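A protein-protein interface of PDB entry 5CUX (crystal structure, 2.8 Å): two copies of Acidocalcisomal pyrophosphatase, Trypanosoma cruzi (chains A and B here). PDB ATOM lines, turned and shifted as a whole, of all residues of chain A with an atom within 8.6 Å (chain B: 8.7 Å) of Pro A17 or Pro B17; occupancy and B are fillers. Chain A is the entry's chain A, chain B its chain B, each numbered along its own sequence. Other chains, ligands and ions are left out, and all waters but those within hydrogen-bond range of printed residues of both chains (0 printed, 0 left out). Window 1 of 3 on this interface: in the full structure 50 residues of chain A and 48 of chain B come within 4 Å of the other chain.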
ATOM      1  N   PHE A  14      -7.524  38.721  11.908  1.00  0.00           N
ATOM      2  CA  PHE A  14      -6.528  37.679  11.647  1.00  0.00           C
ATOM      3  C   PHE A  14      -6.597  37.165  10.227  1.00  0.00           C
ATOM      4  O   PHE A  14      -7.496  36.390   9.893  1.00  0.00           O
ATOM      5  CB  PHE A  14      -6.703  36.476  12.591  1.00  0.00           C
ATOM      6  CG  PHE A  14      -5.845  36.528  13.823  1.00  0.00           C
ATOM      7  CD1 PHE A  14      -5.217  37.712  14.216  1.00  0.00           C
ATOM      8  CD2 PHE A  14      -5.715  35.403  14.631  1.00  0.00           C
ATOM      9  CE1 PHE A  14      -4.479  37.773  15.399  1.00  0.00           C
ATOM     10  CE2 PHE A  14      -4.981  35.452  15.812  1.00  0.00           C
ATOM     11  CZ  PHE A  14      -4.363  36.640  16.196  1.00  0.00           C
ATOM     12  N   ALA A  15      -5.647  37.572   9.389  1.00  0.00           N
ATOM     13  CA  ALA A  15      -5.643  37.092   8.011  1.00  0.00           C
ATOM     14  C   ALA A  15      -5.264  35.598   7.983  1.00  0.00           C
ATOM     15  O   ALA A  15      -4.274  35.185   8.610  1.00  0.00           O
ATOM     16  CB  ALA A  15      -4.661  37.914   7.156  1.00  0.00           C
ATOM     17  N   VAL A  16      -6.089  34.803   7.290  1.00  0.00           N
ATOM     18  CA  VAL A  16      -5.865  33.365   7.120  1.00  0.00           C
ATOM     19  C   VAL A  16      -4.956  33.271   5.903  1.00  0.00           C
ATOM     20  O   VAL A  16      -5.423  33.324   4.753  1.00  0.00           O
ATOM     21  CB  VAL A  16      -7.170  32.601   6.799  1.00  0.00           C
ATOM     22  CG1 VAL A  16      -6.860  31.116   6.608  1.00  0.00           C
ATOM     23  CG2 VAL A  16      -8.196  32.817   7.905  1.00  0.00           C
ATOM     24  N   PRO A  17      -3.638  33.122   6.140  1.00  0.00           N
ATOM     25  CA  PRO A  17      -2.644  33.030   5.059  1.00  0.00           C
ATOM     26  C   PRO A  17      -2.896  31.950   3.987  1.00  0.00           C
ATOM     27  O   PRO A  17      -3.791  32.089   3.132  1.00  0.00           O
ATOM     28  CB  PRO A  17      -1.319  32.838   5.822  1.00  0.00           C
ATOM     29  CG  PRO A  17      -1.743  32.155   7.096  1.00  0.00           C
ATOM     30  CD  PRO A  17      -3.021  32.866   7.459  1.00  0.00           C
ATOM     31  N   TYR A  18      -2.093  30.885   4.055  1.00  0.00           N
ATOM     32  CA  TYR A  18      -2.141  29.749   3.134  1.00  0.00           C
ATOM     33  C   TYR A  18      -3.516  29.250   2.666  1.00  0.00           C
ATOM     34  O   TYR A  18      -4.566  29.489   3.296  1.00  0.00           O
ATOM     35  CB  TYR A  18      -1.367  28.572   3.744  1.00  0.00           C
ATOM     36  CG  TYR A  18      -0.163  28.166   2.930  1.00  0.00           C
ATOM     37  CD1 TYR A  18       0.924  29.037   2.787  1.00  0.00           C
ATOM     38  CD2 TYR A  18      -0.139  26.939   2.240  1.00  0.00           C
ATOM     39  CE1 TYR A  18       2.004  28.703   1.971  1.00  0.00           C
ATOM     40  CE2 TYR A  18       0.936  26.594   1.423  1.00  0.00           C
ATOM     41  CZ  TYR A  18       2.004  27.484   1.289  1.00  0.00           C
ATOM     42  OH  TYR A  18       3.065  27.180   0.461  1.00  0.00           O
ATOM     43  N   HIS A  19      -3.483  28.543   1.543  1.00  0.00           N
ATOM     44  CA  HIS A  19      -4.684  27.983   0.971  1.00  0.00           C
ATOM     45  C   HIS A  19      -4.763  26.551   1.427  1.00  0.00           C
ATOM     46  O   HIS A  19      -3.744  25.889   1.617  1.00  0.00           O
ATOM     47  CB  HIS A  19      -4.614  28.057  -0.545  1.00  0.00           C
ATOM     48  CG  HIS A  19      -4.461  29.450  -1.068  1.00  0.00           C
ATOM     49  ND1 HIS A  19      -4.309  29.730  -2.410  1.00  0.00           N
ATOM     50  CD2 HIS A  19      -4.462  30.646  -0.430  1.00  0.00           C
ATOM     51  CE1 HIS A  19      -4.225  31.039  -2.574  1.00  0.00           C
ATOM     52  NE2 HIS A  19      -4.315  31.616  -1.389  1.00  0.00           N
ATOM     53  N   GLN A  20      -5.982  26.076   1.621  1.00  0.00           N
ATOM     54  CA  GLN A  20      -6.177  24.716   2.066  1.00  0.00           C
ATOM     55  C   GLN A  20      -5.822  23.770   0.930  1.00  0.00           C
ATOM     56  O   GLN A  20      -6.164  24.007  -0.213  1.00  0.00           O
ATOM     57  CB  GLN A  20      -7.625  24.513   2.519  1.00  0.00           C
ATOM     58  CG  GLN A  20      -7.958  23.075   2.744  1.00  0.00           C
ATOM     59  CD  GLN A  20      -9.261  22.875   3.450  1.00  0.00           C
ATOM     60  OE1 GLN A  20     -10.282  23.413   3.053  1.00  0.00           O
ATOM     61  NE2 GLN A  20      -9.240  22.077   4.507  1.00  0.00           N
ATOM     62  N   ASP A  44      -4.214  22.871  -4.518  1.00  0.00           N
ATOM     63  CA  ASP A  44      -4.576  24.114  -3.849  1.00  0.00           C
ATOM     64  C   ASP A  44      -6.111  24.259  -4.015  1.00  0.00           C
ATOM     65  O   ASP A  44      -6.617  24.263  -5.131  1.00  0.00           O
ATOM     66  CB  ASP A  44      -3.845  25.270  -4.541  1.00  0.00           C
ATOM     67  CG  ASP A  44      -4.013  26.589  -3.825  1.00  0.00           C
ATOM     68  OD1 ASP A  44      -5.184  27.034  -3.668  1.00  0.00           O
ATOM     69  OD2 ASP A  44      -2.963  27.163  -3.427  1.00  0.00           O
ATOM     70  N   GLU A  46      -7.848  26.749  -3.694  1.00  0.00           N
ATOM     71  CA  GLU A  46      -8.190  28.048  -4.267  1.00  0.00           C
ATOM     72  C   GLU A  46      -7.894  27.965  -5.765  1.00  0.00           C
ATOM     73  O   GLU A  46      -8.783  27.792  -6.601  1.00  0.00           O
ATOM     74  CB  GLU A  46      -7.317  29.159  -3.675  1.00  0.00           C
ATOM     75  CG  GLU A  46      -7.388  29.302  -2.173  1.00  0.00           C
ATOM     76  CD  GLU A  46      -8.797  29.624  -1.690  1.00  0.00           C
ATOM     77  OE1 GLU A  46      -9.726  28.844  -2.032  1.00  0.00           O
ATOM     78  OE2 GLU A  46      -8.978  30.643  -0.971  1.00  0.00           O
ATOM     79  N   LEU A  66      -7.794  25.602  11.557  1.00  0.00           N
ATOM     80  CA  LEU A  66      -7.354  26.935  11.865  1.00  0.00           C
ATOM     81  C   LEU A  66      -7.663  27.495  13.264  1.00  0.00           C
ATOM     82  O   LEU A  66      -6.803  28.125  13.880  1.00  0.00           O
ATOM     83  CB  LEU A  66      -7.842  27.825  10.727  1.00  0.00           C
ATOM     84  CG  LEU A  66      -7.713  27.104   9.333  1.00  0.00           C
ATOM     85  CD1 LEU A  66      -7.933  28.138   8.213  1.00  0.00           C
ATOM     86  CD2 LEU A  66      -6.327  26.438   9.116  1.00  0.00           C
ATOM     87  N   PHE B  14       5.866  23.421   1.404  1.00  0.00           N
ATOM     88  CA  PHE B  14       4.669  24.236   1.644  1.00  0.00           C
ATOM     89  C   PHE B  14       4.633  24.705   3.099  1.00  0.00           C
ATOM     90  O   PHE B  14       3.954  24.117   3.946  1.00  0.00           O
ATOM     91  CB  PHE B  14       3.394  23.439   1.301  1.00  0.00           C
ATOM     92  CG  PHE B  14       2.749  23.846  -0.009  1.00  0.00           C
ATOM     93  CD1 PHE B  14       3.450  24.603  -0.949  1.00  0.00           C
ATOM     94  CD2 PHE B  14       1.437  23.490  -0.293  1.00  0.00           C
ATOM     95  CE1 PHE B  14       2.849  25.000  -2.145  1.00  0.00           C
ATOM     96  CE2 PHE B  14       0.833  23.884  -1.488  1.00  0.00           C
ATOM     97  CZ  PHE B  14       1.537  24.640  -2.413  1.00  0.00           C
ATOM     98  N   ALA B  15       5.380  25.773   3.371  1.00  0.00           N
ATOM     99  CA  ALA B  15       5.474  26.354   4.709  1.00  0.00           C
ATOM    100  C   ALA B  15       4.108  26.644   5.331  1.00  0.00           C
ATOM    101  O   ALA B  15       3.285  27.375   4.758  1.00  0.00           O
ATOM    102  CB  ALA B  15       6.311  27.649   4.665  1.00  0.00           C
ATOM    103  N   VAL B  16       3.868  26.049   6.498  1.00  0.00           N
ATOM    104  CA  VAL B  16       2.622  26.283   7.213  1.00  0.00           C
ATOM    105  C   VAL B  16       2.780  27.699   7.787  1.00  0.00           C
ATOM    106  O   VAL B  16       3.672  27.955   8.616  1.00  0.00           O
ATOM    107  CB  VAL B  16       2.426  25.281   8.381  1.00  0.00           C
ATOM    108  CG1 VAL B  16       1.012  25.420   8.934  1.00  0.00           C
ATOM    109  CG2 VAL B  16       2.721  23.845   7.922  1.00  0.00           C
ATOM    110  N   PRO B  17       1.935  28.643   7.336  1.00  0.00           N
ATOM    111  CA  PRO B  17       2.038  30.016   7.839  1.00  0.00           C
ATOM    112  C   PRO B  17       1.574  30.200   9.307  1.00  0.00           C
ATOM    113  O   PRO B  17       2.182  29.661  10.250  1.00  0.00           O
ATOM    114  CB  PRO B  17       1.203  30.809   6.824  1.00  0.00           C
ATOM    115  CG  PRO B  17       0.133  29.832   6.444  1.00  0.00           C
ATOM    116  CD  PRO B  17       0.880  28.525   6.309  1.00  0.00           C
ATOM    117  N   TYR B  18       0.496  30.967   9.476  1.00  0.00           N
ATOM    118  CA  TYR B  18      -0.090  31.274  10.775  1.00  0.00           C
ATOM    119  C   TYR B  18      -0.086  30.153  11.829  1.00  0.00           C
ATOM    120  O   TYR B  18       0.090  28.965  11.507  1.00  0.00           O
ATOM    121  CB  TYR B  18      -1.514  31.788  10.548  1.00  0.00           C
ATOM    122  CG  TYR B  18      -1.771  33.113  11.225  1.00  0.00           C
ATOM    123  CD1 TYR B  18      -1.276  33.362  12.520  1.00  0.00           C
ATOM    124  CD2 TYR B  18      -2.510  34.121  10.589  1.00  0.00           C
ATOM    125  CE1 TYR B  18      -1.509  34.580  13.167  1.00  0.00           C
ATOM    126  CE2 TYR B  18      -2.751  35.349  11.226  1.00  0.00           C
ATOM    127  CZ  TYR B  18      -2.244  35.567  12.517  1.00  0.00           C
ATOM    128  OH  TYR B  18      -2.461  36.762  13.165  1.00  0.00           O
ATOM    129  N   HIS B  19      -0.258  30.555  13.089  1.00  0.00           N
ATOM    130  CA  HIS B  19      -0.292  29.626  14.219  1.00  0.00           C
ATOM    131  C   HIS B  19      -1.739  29.270  14.464  1.00  0.00           C
ATOM    132  O   HIS B  19      -2.618  30.087  14.247  1.00  0.00           O
ATOM    133  CB  HIS B  19       0.224  30.278  15.489  1.00  0.00           C
ATOM    134  CG  HIS B  19       1.575  30.892  15.357  1.00  0.00           C
ATOM    135  ND1 HIS B  19       2.177  31.581  16.387  1.00  0.00           N
ATOM    136  CD2 HIS B  19       2.454  30.903  14.329  1.00  0.00           C
ATOM    137  CE1 HIS B  19       3.371  31.988  15.999  1.00  0.00           C
ATOM    138  NE2 HIS B  19       3.562  31.590  14.754  1.00  0.00           N
ATOM    139  N   GLN B  20      -1.986  28.062  14.936  1.00  0.00           N
ATOM    140  CA  GLN B  20      -3.351  27.643  15.198  1.00  0.00           C
ATOM    141  C   GLN B  20      -3.807  28.374  16.425  1.00  0.00           C
ATOM    142  O   GLN B  20      -3.008  28.672  17.283  1.00  0.00           O
ATOM    143  CB  GLN B  20      -3.424  26.135  15.438  1.00  0.00           C
ATOM    144  CG  GLN B  20      -4.849  25.606  15.526  1.00  0.00           C
ATOM    145  CD  GLN B  20      -4.901  24.128  15.811  1.00  0.00           C
ATOM    146  OE1 GLN B  20      -3.939  23.574  16.337  1.00  0.00           O
ATOM    147  NE2 GLN B  20      -6.029  23.478  15.481  1.00  0.00           N
ATOM    148  N   ASP B  44      -2.936  31.951  21.047  1.00  0.00           N
ATOM    149  CA  ASP B  44      -2.063  31.412  20.013  1.00  0.00           C
ATOM    150  C   ASP B  44      -1.500  30.099  20.581  1.00  0.00           C
ATOM    151  O   ASP B  44      -1.081  30.047  21.743  1.00  0.00           O
ATOM    152  CB  ASP B  44      -0.943  32.404  19.714  1.00  0.00           C
ATOM    153  CG  ASP B  44       0.028  31.889  18.681  1.00  0.00           C
ATOM    154  OD1 ASP B  44       0.760  30.913  18.981  1.00  0.00           O
ATOM    155  OD2 ASP B  44       0.051  32.465  17.573  1.00  0.00           O
ATOM    156  N   GLU B  46       1.246  28.468  19.713  1.00  0.00           N
ATOM    157  CA  GLU B  46       2.713  28.441  19.769  1.00  0.00           C
ATOM    158  C   GLU B  46       3.128  29.382  20.886  1.00  0.00           C
ATOM    159  O   GLU B  46       3.580  28.940  21.955  1.00  0.00           O
ATOM    160  CB  GLU B  46       3.312  28.946  18.472  1.00  0.00           C
ATOM    161  CG  GLU B  46       2.693  28.280  17.270  1.00  0.00           C
ATOM    162  CD  GLU B  46       3.724  27.586  16.391  1.00  0.00           C
ATOM    163  OE1 GLU B  46       4.645  28.291  15.878  1.00  0.00           O
ATOM    164  OE2 GLU B  46       3.599  26.339  16.222  1.00  0.00           O
ATOM    165  N   LEU B  66      -5.499  22.348   7.589  1.00  0.00           N
ATOM    166  CA  LEU B  66      -4.511  22.676   6.584  1.00  0.00           C
ATOM    167  C   LEU B  66      -4.523  21.777   5.361  1.00  0.00           C
ATOM    168  O   LEU B  66      -4.591  22.290   4.250  1.00  0.00           O
ATOM    169  CB  LEU B  66      -3.125  22.693   7.209  1.00  0.00           C
ATOM    170  CG  LEU B  66      -3.035  23.136   8.678  1.00  0.00           C
ATOM    171  CD1 LEU B  66      -1.589  23.543   8.945  1.00  0.00           C
ATOM    172  CD2 LEU B  66      -3.983  24.281   9.001  1.00  0.00           C
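Among the printed residues, pairs that only touch across the chains: Phe A14 with Tyr B18 (3.1 Å), Ala A15 with Tyr B18 (2.9 Å), Pro A17 with Pro B17 (3.1 Å), Pro A17 with Tyr B18 (3.4 Å), Tyr A18 with Phe B14 (3.0 Å), Tyr A18 with Ala B15 (3.3 Å), Tyr A18 with Pro B17 (3.3 Å), Gln A20 with Leu B66 (3.6 Å), Leu A66 with Gln B20 (3.6 Å) and Leu A66 with Leu B66 (3.2 Å).
Phe A14 touches Tyr B18, and with the chains exchanged Tyr A18 touches Phe B14. Pro A17 touches its own counterpart, Pro B17. Pro A17 touches Tyr B18, and with the chains exchanged Tyr A18 touches Pro B17. Gln A20 touches Leu B66, and with the chains exchanged Leu A66 touches Gln B20.
Pro A17 touches just these residues of chain B: Pro B17 (3.1 Å) and Tyr B18 (3.4 Å). Pro B17 touches two residues of chain A. Of the printed residues of chain A, Phe B14 touches Tyr A18. Printed residues of chain A within 4 Å of Ala B15: Tyr A18. The nearest printed residue of chain B that does not touch Pro A17 is His B19 (6.4 Å).
Of the 10 printed residues of chain B, 6 touch a printed residue of chain A. Hydrophobic or aromatic side chains of chain B that line the printed part of chain A: Phe B14, Pro B17, Tyr B18 and Leu B66. Printed residues of chain A that touch a printed residue of chain B: Phe A14, Ala A15, Pro A17, Tyr A18, Gln A20 and Leu A66. Hydrophobic or aromatic side chains of chain A that line the printed part of chain B: Phe A14, Pro A17, Tyr A18 and Leu A66. Among the printed residues, no Asp or Glu carboxylate lies within 4 Å of a Lys or Arg side-chain nitrogen of the other chain.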
